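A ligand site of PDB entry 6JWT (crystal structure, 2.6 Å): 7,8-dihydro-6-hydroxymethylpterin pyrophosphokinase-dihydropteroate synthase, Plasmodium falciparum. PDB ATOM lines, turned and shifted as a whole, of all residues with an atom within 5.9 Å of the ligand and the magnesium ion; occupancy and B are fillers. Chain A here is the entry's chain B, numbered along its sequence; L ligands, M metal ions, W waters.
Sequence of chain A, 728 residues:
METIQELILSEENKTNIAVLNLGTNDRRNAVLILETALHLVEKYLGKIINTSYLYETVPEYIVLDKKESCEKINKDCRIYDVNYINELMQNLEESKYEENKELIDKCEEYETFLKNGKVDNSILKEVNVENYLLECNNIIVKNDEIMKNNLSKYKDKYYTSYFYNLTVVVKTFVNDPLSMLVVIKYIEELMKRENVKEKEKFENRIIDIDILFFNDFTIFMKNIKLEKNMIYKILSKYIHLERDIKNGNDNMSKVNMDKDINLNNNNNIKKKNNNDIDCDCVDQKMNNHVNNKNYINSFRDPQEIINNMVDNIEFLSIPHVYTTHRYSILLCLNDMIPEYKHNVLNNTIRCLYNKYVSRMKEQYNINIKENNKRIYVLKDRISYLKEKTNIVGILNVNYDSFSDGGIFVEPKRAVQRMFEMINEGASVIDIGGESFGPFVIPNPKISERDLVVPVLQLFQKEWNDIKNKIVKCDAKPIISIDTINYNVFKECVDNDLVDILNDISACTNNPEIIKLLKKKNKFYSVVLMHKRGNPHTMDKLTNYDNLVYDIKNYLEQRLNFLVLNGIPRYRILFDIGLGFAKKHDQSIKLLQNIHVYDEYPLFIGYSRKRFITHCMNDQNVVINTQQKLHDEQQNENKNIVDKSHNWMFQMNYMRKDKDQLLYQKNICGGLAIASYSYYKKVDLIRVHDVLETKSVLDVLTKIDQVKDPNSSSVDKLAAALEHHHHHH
The side-chain hydroxyl of Ser 317 is in hydrogen-bond range of the backbone carbonyl oxygen of Pro 319, 3.1 Å away. ND1 of His 320 is in hydrogen-bond range of N of Tyr 322, 3.2 Å away. The backbone NH (N) of His 320 sits at hydrogen-bond distance from the backbone carbonyl oxygen (O) of Leu 212 (3.4 Å). NZ of Lys 185 lies within salt-bridge range of OE1 of Glu 188.
O of Phe 315 lies close to N1 of the ligand. CD1 of Leu 181 touches C9 of the ligand, at 3.6 Å. Lys 185 touches the ligand (CE to O13, 3.9 Å). CA of Ile 313 touches O13 of the ligand, 3.8 Å away. Leu 316 touches the ligand (CA to C6, 3.4 Å). Hydrophobic or aromatic side chains within 4 Å of the ligand: Leu 181, Ile 211, Phe 315 and His 320. The nearest printed residue that does not touch the ligand is Ile 318 (4.2 Å).
The magnesium ion is bound by OD1 of Asp 210 (2.0 Å), O4 of the ligand (2.2 Å), OD1 of Asp 208 (2.3 Å), O7 of the ligand (2.3 Å), water W1 (2.4 Å) and OD2 of Asp 208 (2.6 Å). The magnesium ion has six donor atoms within binding distance.
Two residues have an atom within 4 Å of the magnesium ion: Asp 208 and Asp 210. The nearest printed residue that does not touch the magnesium ion is His 320 (4.6 Å).
The backbone NH of Ser 317 is in hydrogen-bond range of a nitrogen (N2) of the ligand (2.7 Å). O of Ser 317 lies within hydrogen-bond range of N3 of the ligand, 2.8 Å away. The backbone NH of Ile 211 is in hydrogen-bond range of a nitrogen (N4) of the ligand (3.0 Å). A nitrogen (N3) of the ligand lies within hydrogen-bond range of the backbone carbonyl oxygen (O) of Ile 211, at 2.8 Å. The backbone carbonyl oxygen of Asn 312 is in hydrogen-bond range of an oxygen (O12) of the ligand, 2.9 Å away. A ring nitrogen (NE2) of His 320 lies close to an oxygen (O7) of the ligand (3.1 Å).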
ATOM      1  N   ASN A 143      17.231  30.700 -16.873  1.00  0.00           N
ATOM      2  CA  ASN A 143      18.095  31.764 -16.357  1.00  0.00           C
ATOM      3  C   ASN A 143      18.210  32.909 -17.371  1.00  0.00           C
ATOM      4  O   ASN A 143      18.463  34.047 -16.955  1.00  0.00           O
ATOM      5  CB  ASN A 143      19.492  31.262 -16.002  1.00  0.00           C
ATOM      6  CG  ASN A 143      19.550  30.496 -14.702  1.00  0.00           C
ATOM      7  OD1 ASN A 143      18.826  30.791 -13.768  1.00  0.00           O
ATOM      8  ND2 ASN A 143      20.442  29.512 -14.631  1.00  0.00           N
ATOM      9  N   LEU A 181      29.645  20.138  -1.263  1.00  0.00           N
ATOM     10  CA  LEU A 181      28.941  21.386  -1.499  1.00  0.00           C
ATOM     11  C   LEU A 181      28.561  22.050  -0.182  1.00  0.00           C
ATOM     12  O   LEU A 181      28.589  23.274  -0.068  1.00  0.00           O
ATOM     13  CB  LEU A 181      27.733  21.100  -2.393  1.00  0.00           C
ATOM     14  CG  LEU A 181      27.004  22.329  -2.950  1.00  0.00           C
ATOM     15  CD1 LEU A 181      27.964  23.425  -3.383  1.00  0.00           C
ATOM     16  CD2 LEU A 181      26.083  21.945  -4.104  1.00  0.00           C
ATOM     17  N   LYS A 185      29.901  25.581   0.959  1.00  0.00           N
ATOM     18  CA  LYS A 185      28.972  26.616   1.386  1.00  0.00           C
ATOM     19  C   LYS A 185      29.379  27.203   2.735  1.00  0.00           C
ATOM     20  O   LYS A 185      29.221  28.407   2.952  1.00  0.00           O
ATOM     21  CB  LYS A 185      27.533  26.077   1.398  1.00  0.00           C
ATOM     22  CG  LYS A 185      26.813  26.170   0.067  1.00  0.00           C
ATOM     23  CD  LYS A 185      26.675  27.606  -0.464  1.00  0.00           C
ATOM     24  CE  LYS A 185      26.322  27.661  -1.939  1.00  0.00           C
ATOM     25  NZ  LYS A 185      26.003  29.060  -2.349  1.00  0.00           N
ATOM     26  N   GLU A 188      32.302  29.531   2.021  1.00  0.00           N
ATOM     27  CA  GLU A 188      31.805  30.789   1.485  1.00  0.00           C
ATOM     28  C   GLU A 188      31.336  31.668   2.635  1.00  0.00           C
ATOM     29  O   GLU A 188      31.834  32.781   2.810  1.00  0.00           O
ATOM     30  CB  GLU A 188      30.660  30.538   0.493  1.00  0.00           C
ATOM     31  CG  GLU A 188      31.091  30.481  -0.972  1.00  0.00           C
ATOM     32  CD  GLU A 188      30.033  29.936  -1.925  1.00  0.00           C
ATOM     33  OE1 GLU A 188      29.645  28.770  -1.753  1.00  0.00           O
ATOM     34  OE2 GLU A 188      29.603  30.676  -2.847  1.00  0.00           O
ATOM     35  N   ASP A 208      32.381  32.696  -5.021  1.00  0.00           N
ATOM     36  CA  ASP A 208      31.453  31.702  -5.521  1.00  0.00           C
ATOM     37  C   ASP A 208      32.282  30.478  -5.893  1.00  0.00           C
ATOM     38  O   ASP A 208      33.082  30.539  -6.814  1.00  0.00           O
ATOM     39  CB  ASP A 208      30.615  32.253  -6.688  1.00  0.00           C
ATOM     40  CG  ASP A 208      29.598  31.291  -7.300  1.00  0.00           C
ATOM     41  OD1 ASP A 208      29.248  30.282  -6.642  1.00  0.00           O
ATOM     42  OD2 ASP A 208      29.146  31.557  -8.428  1.00  0.00           O
ATOM     43  N   ILE A 209      32.090  29.384  -5.151  1.00  0.00           N
ATOM     44  CA  ILE A 209      32.847  28.165  -5.375  1.00  0.00           C
ATOM     45  C   ILE A 209      31.856  27.104  -5.836  1.00  0.00           C
ATOM     46  O   ILE A 209      30.977  26.706  -5.086  1.00  0.00           O
ATOM     47  CB  ILE A 209      33.585  27.726  -4.087  1.00  0.00           C
ATOM     48  CG1 ILE A 209      34.429  28.857  -3.496  1.00  0.00           C
ATOM     49  CG2 ILE A 209      34.404  26.486  -4.337  1.00  0.00           C
ATOM     50  CD1 ILE A 209      34.749  28.708  -2.017  1.00  0.00           C
ATOM     51  N   ASP A 210      32.009  26.676  -7.086  1.00  0.00           N
ATOM     52  CA  ASP A 210      31.118  25.696  -7.675  1.00  0.00           C
ATOM     53  C   ASP A 210      31.907  24.399  -7.798  1.00  0.00           C
ATOM     54  O   ASP A 210      33.119  24.441  -7.815  1.00  0.00           O
ATOM     55  CB  ASP A 210      30.637  26.119  -9.067  1.00  0.00           C
ATOM     56  CG  ASP A 210      30.018  27.501  -9.081  1.00  0.00           C
ATOM     57  OD1 ASP A 210      29.060  27.740  -8.292  1.00  0.00           O
ATOM     58  OD2 ASP A 210      30.500  28.351  -9.854  1.00  0.00           O
ATOM     59  N   ILE A 211      31.184  23.277  -7.852  1.00  0.00           N
ATOM     60  CA  ILE A 211      31.779  21.996  -8.179  1.00  0.00           C
ATOM     61  C   ILE A 211      31.486  21.759  -9.650  1.00  0.00           C
ATOM     62  O   ILE A 211      30.389  22.046 -10.094  1.00  0.00           O
ATOM     63  CB  ILE A 211      31.175  20.881  -7.316  1.00  0.00           C
ATOM     64  CG1 ILE A 211      31.165  21.255  -5.834  1.00  0.00           C
ATOM     65  CG2 ILE A 211      31.895  19.560  -7.579  1.00  0.00           C
ATOM     66  CD1 ILE A 211      31.009  20.078  -4.910  1.00  0.00           C
ATOM     67  N   LEU A 212      32.474  21.256 -10.385  1.00  0.00           N
ATOM     68  CA  LEU A 212      32.341  21.097 -11.822  1.00  0.00           C
ATOM     69  C   LEU A 212      32.329  19.607 -12.136  1.00  0.00           C
ATOM     70  O   LEU A 212      31.666  19.156 -13.055  1.00  0.00           O
ATOM     71  CB  LEU A 212      33.515  21.777 -12.544  1.00  0.00           C
ATOM     72  CG  LEU A 212      33.707  23.270 -12.271  1.00  0.00           C
ATOM     73  CD1 LEU A 212      35.062  23.729 -12.780  1.00  0.00           C
ATOM     74  CD2 LEU A 212      32.602  24.102 -12.900  1.00  0.00           C
ATOM     75  N   ASN A 312      20.253  27.783   0.740  1.00  0.00           N
ATOM     76  CA  ASN A 312      21.252  28.058  -0.292  1.00  0.00           C
ATOM     77  C   ASN A 312      21.362  26.960  -1.352  1.00  0.00           C
ATOM     78  O   ASN A 312      21.610  27.262  -2.520  1.00  0.00           O
ATOM     79  CB  ASN A 312      22.624  28.395   0.312  1.00  0.00           C
ATOM     80  CG  ASN A 312      22.717  29.820   0.826  1.00  0.00           C
ATOM     81  OD1 ASN A 312      21.871  30.663   0.510  1.00  0.00           O
ATOM     82  ND2 ASN A 312      23.744  30.111   1.606  1.00  0.00           N
ATOM     83  N   ILE A 313      21.174  25.690  -0.958  1.00  0.00           N
ATOM     84  CA  ILE A 313      21.389  24.554  -1.842  1.00  0.00           C
ATOM     85  C   ILE A 313      20.061  24.134  -2.463  1.00  0.00           C
ATOM     86  O   ILE A 313      19.409  23.188  -1.997  1.00  0.00           O
ATOM     87  CB  ILE A 313      22.074  23.407  -1.078  1.00  0.00           C
ATOM     88  CG1 ILE A 313      23.328  23.894  -0.358  1.00  0.00           C
ATOM     89  CG2 ILE A 313      22.377  22.238  -2.002  1.00  0.00           C
ATOM     90  CD1 ILE A 313      23.438  23.394   1.067  1.00  0.00           C
ATOM     91  N   GLU A 314      19.675  24.826  -3.534  1.00  0.00           N
ATOM     92  CA  GLU A 314      18.409  24.612  -4.217  1.00  0.00           C
ATOM     93  C   GLU A 314      18.418  23.239  -4.902  1.00  0.00           C
ATOM     94  O   GLU A 314      17.383  22.571  -4.941  1.00  0.00           O
ATOM     95  CB  GLU A 314      18.155  25.746  -5.220  1.00  0.00           C
ATOM     96  CG  GLU A 314      16.681  26.022  -5.508  1.00  0.00           C
ATOM     97  CD  GLU A 314      16.078  27.235  -4.822  1.00  0.00           C
ATOM     98  OE1 GLU A 314      16.662  28.334  -4.933  1.00  0.00           O
ATOM     99  OE2 GLU A 314      15.010  27.088  -4.181  1.00  0.00           O
ATOM    100  N   PHE A 315      19.584  22.842  -5.430  1.00  0.00           N
ATOM    101  CA  PHE A 315      19.769  21.585  -6.151  1.00  0.00           C
ATOM    102  C   PHE A 315      21.259  21.259  -6.249  1.00  0.00           C
ATOM    103  O   PHE A 315      22.076  21.972  -5.687  1.00  0.00           O
ATOM    104  CB  PHE A 315      19.108  21.608  -7.540  1.00  0.00           C
ATOM    105  CG  PHE A 315      19.611  22.642  -8.517  1.00  0.00           C
ATOM    106  CD1 PHE A 315      19.279  23.978  -8.392  1.00  0.00           C
ATOM    107  CD2 PHE A 315      20.401  22.267  -9.604  1.00  0.00           C
ATOM    108  CE1 PHE A 315      19.730  24.920  -9.305  1.00  0.00           C
ATOM    109  CE2 PHE A 315      20.853  23.209 -10.517  1.00  0.00           C
ATOM    110  CZ  PHE A 315      20.525  24.532 -10.361  1.00  0.00           C
ATOM    111  N   LEU A 316      21.594  20.160  -6.945  1.00  0.00           N
ATOM    112  CA  LEU A 316      22.963  19.762  -7.201  1.00  0.00           C
ATOM    113  C   LEU A 316      23.100  19.158  -8.600  1.00  0.00           C
ATOM    114  O   LEU A 316      22.544  18.091  -8.879  1.00  0.00           O
ATOM    115  CB  LEU A 316      23.457  18.756  -6.150  1.00  0.00           C
ATOM    116  CG  LEU A 316      24.808  18.126  -6.483  1.00  0.00           C
ATOM    117  CD1 LEU A 316      25.939  19.136  -6.351  1.00  0.00           C
ATOM    118  CD2 LEU A 316      25.065  16.899  -5.628  1.00  0.00           C
ATOM    119  N   SER A 317      23.915  19.832  -9.431  1.00  0.00           N
ATOM    120  CA  SER A 317      24.192  19.349 -10.781  1.00  0.00           C
ATOM    121  C   SER A 317      25.685  19.038 -10.956  1.00  0.00           C
ATOM    122  O   SER A 317      26.541  19.897 -10.731  1.00  0.00           O
ATOM    123  CB  SER A 317      23.703  20.342 -11.801  1.00  0.00           C
ATOM    124  OG  SER A 317      23.945  19.837 -13.097  1.00  0.00           O
ATOM    125  N   ILE A 318      25.970  17.788 -11.334  1.00  0.00           N
ATOM    126  CA  ILE A 318      27.309  17.277 -11.583  1.00  0.00           C
ATOM    127  C   ILE A 318      27.257  16.495 -12.894  1.00  0.00           C
ATOM    128  O   ILE A 318      26.548  15.502 -12.972  1.00  0.00           O
ATOM    129  CB  ILE A 318      27.791  16.361 -10.440  1.00  0.00           C
ATOM    130  CG1 ILE A 318      27.777  17.041  -9.061  1.00  0.00           C
ATOM    131  CG2 ILE A 318      29.134  15.729 -10.780  1.00  0.00           C
ATOM    132  CD1 ILE A 318      29.046  17.754  -8.685  1.00  0.00           C
ATOM    133  N   PRO A 319      27.974  16.918 -13.964  1.00  0.00           N
ATOM    134  CA  PRO A 319      28.821  18.119 -13.915  1.00  0.00           C
ATOM    135  C   PRO A 319      27.945  19.353 -13.772  1.00  0.00           C
ATOM    136  O   PRO A 319      26.785  19.328 -14.176  1.00  0.00           O
ATOM    137  CB  PRO A 319      29.431  18.179 -15.313  1.00  0.00           C
ATOM    138  CG  PRO A 319      29.252  16.792 -15.911  1.00  0.00           C
ATOM    139  CD  PRO A 319      27.991  16.255 -15.267  1.00  0.00           C
ATOM    140  N   HIS A 320      28.504  20.414 -13.185  1.00  0.00           N
ATOM    141  CA  HIS A 320      27.869  21.716 -13.084  1.00  0.00           C
ATOM    142  C   HIS A 320      27.207  22.049 -14.410  1.00  0.00           C
ATOM    143  O   HIS A 320      27.673  21.629 -15.471  1.00  0.00           O
ATOM    144  CB  HIS A 320      28.928  22.775 -12.748  1.00  0.00           C
ATOM    145  CG  HIS A 320      28.377  24.072 -12.263  1.00  0.00           C
ATOM    146  ND1 HIS A 320      27.960  25.069 -13.140  1.00  0.00           N
ATOM    147  CD2 HIS A 320      28.187  24.550 -11.012  1.00  0.00           C
ATOM    148  CE1 HIS A 320      27.543  26.113 -12.436  1.00  0.00           C
ATOM    149  NE2 HIS A 320      27.659  25.816 -11.115  1.00  0.00           N
ATOM    150  N   VAL A 321      26.117  22.800 -14.314  1.00  0.00           N
ATOM    151  CA  VAL A 321      25.268  23.130 -15.453  1.00  0.00           C
ATOM    152  C   VAL A 321      26.098  23.860 -16.510  1.00  0.00           C
ATOM    153  O   VAL A 321      26.158  23.425 -17.665  1.00  0.00           O
ATOM    154  CB  VAL A 321      24.031  23.908 -14.940  1.00  0.00           C
ATOM    155  CG1 VAL A 321      23.453  24.889 -15.939  1.00  0.00           C
ATOM    156  CG2 VAL A 321      22.967  22.960 -14.409  1.00  0.00           C
ATOM    157  N   TYR A 322      26.835  24.887 -16.086  1.00  0.00           N
ATOM    158  CA  TYR A 322      27.422  25.847 -17.000  1.00  0.00           C
ATOM    159  C   TYR A 322      28.733  25.356 -17.629  1.00  0.00           C
ATOM    160  O   TYR A 322      29.344  26.087 -18.423  1.00  0.00           O
ATOM    161  CB  TYR A 322      27.453  27.219 -16.334  1.00  0.00           C
ATOM    162  CG  TYR A 322      26.128  27.922 -16.437  1.00  0.00           C
ATOM    163  CD1 TYR A 322      25.803  28.666 -17.571  1.00  0.00           C
ATOM    164  CD2 TYR A 322      25.184  27.830 -15.431  1.00  0.00           C
ATOM    165  CE1 TYR A 322      24.579  29.301 -17.687  1.00  0.00           C
ATOM    166  CE2 TYR A 322      23.949  28.458 -15.529  1.00  0.00           C
ATOM    167  CZ  TYR A 322      23.651  29.202 -16.667  1.00  0.00           C
ATOM    168  OH  TYR A 322      22.440  29.826 -16.797  1.00  0.00           O
ATOM    169  N   ARG A 326      29.770  28.328 -20.495  1.00  0.00           N
ATOM    170  CA  ARG A 326      30.618  29.455 -20.116  1.00  0.00           C
ATOM    171  C   ARG A 326      32.022  29.282 -20.675  1.00  0.00           C
ATOM    172  O   ARG A 326      32.727  28.349 -20.311  1.00  0.00           O
ATOM    173  CB  ARG A 326      30.729  29.600 -18.592  1.00  0.00           C
ATOM    174  CG  ARG A 326      29.498  30.185 -17.929  1.00  0.00           C
ATOM    175  CD  ARG A 326      29.823  31.201 -16.853  1.00  0.00           C
ATOM    176  NE  ARG A 326      28.616  31.383 -16.068  1.00  0.00           N
ATOM    177  CZ  ARG A 326      28.312  30.695 -14.969  1.00  0.00           C
ATOM    178  NH1 ARG A 326      29.147  29.783 -14.496  1.00  0.00           N
ATOM    179  NH2 ARG A 326      27.182  30.931 -14.338  1.00  0.00           N
HETATM  180  P1  LIG L   1      24.166  32.882  -9.585  1.00  0.00           P
HETATM  181  O1  LIG L   1      23.563  32.588 -10.941  1.00  0.00           O
HETATM  182  O2  LIG L   1      23.418  33.967  -8.835  1.00  0.00           O
HETATM  183  O3  LIG L   1      25.668  33.144  -9.668  1.00  0.00           O
HETATM  184  P2  LIG L   1      25.045  30.560  -7.997  1.00  0.00           P
HETATM  185  O4  LIG L   1      26.349  30.714  -8.723  1.00  0.00           O
HETATM  186  O5  LIG L   1      25.007  30.698  -6.510  1.00  0.00           O
HETATM  187  O6  LIG L   1      23.987  31.520  -8.712  1.00  0.00           O
HETATM  188  P3  LIG L   1      24.996  28.128  -9.457  1.00  0.00           P
HETATM  189  O7  LIG L   1      26.454  27.893  -9.213  1.00  0.00           O
HETATM  190  O8  LIG L   1      24.543  28.650 -10.780  1.00  0.00           O
HETATM  191  O9  LIG L   1      24.429  29.133  -8.364  1.00  0.00           O
HETATM  192  O10 LIG L   1      24.185  26.793  -9.087  1.00  0.00           O
HETATM  193  C1  LIG L   1      22.754  26.944  -8.914  1.00  0.00           C
HETATM  194  C2  LIG L   1      22.341  26.656  -7.493  1.00  0.00           C
HETATM  195  O11 LIG L   1      22.285  25.226  -7.265  1.00  0.00           O
HETATM  196  C3  LIG L   1      23.176  27.237  -6.348  1.00  0.00           C
HETATM  197  O12 LIG L   1      22.280  27.670  -5.340  1.00  0.00           O
HETATM  198  C4  LIG L   1      23.986  26.050  -5.812  1.00  0.00           C
HETATM  199  O13 LIG L   1      23.865  25.939  -4.412  1.00  0.00           O
HETATM  200  C5  LIG L   1      23.353  24.819  -6.454  1.00  0.00           C
HETATM  201  N1  LIG L   1      24.237  23.959  -7.250  1.00  0.00           N
HETATM  202  C6  LIG L   1      23.832  22.936  -8.094  1.00  0.00           C
HETATM  203  N2  LIG L   1      24.846  22.292  -8.633  1.00  0.00           N
HETATM  204  C7  LIG L   1      25.967  22.923  -8.117  1.00  0.00           C
HETATM  205  C8  LIG L   1      27.340  22.702  -8.310  1.00  0.00           C
HETATM  206  N3  LIG L   1      27.816  21.729  -9.083  1.00  0.00           N
HETATM  207  N4  LIG L   1      28.192  23.503  -7.633  1.00  0.00           N
HETATM  208  C9  LIG L   1      27.710  24.477  -6.853  1.00  0.00           C
HETATM  209  N5  LIG L   1      26.436  24.779  -6.596  1.00  0.00           N
HETATM  210  C10 LIG L   1      25.607  23.961  -7.265  1.00  0.00           C
HETATM  211 MG    MG M   1      27.887  29.303  -8.151  1.00  0.00          MG
HETATM  212  O   HOH W   1      28.110  30.346 -10.312  1.00  0.00           O
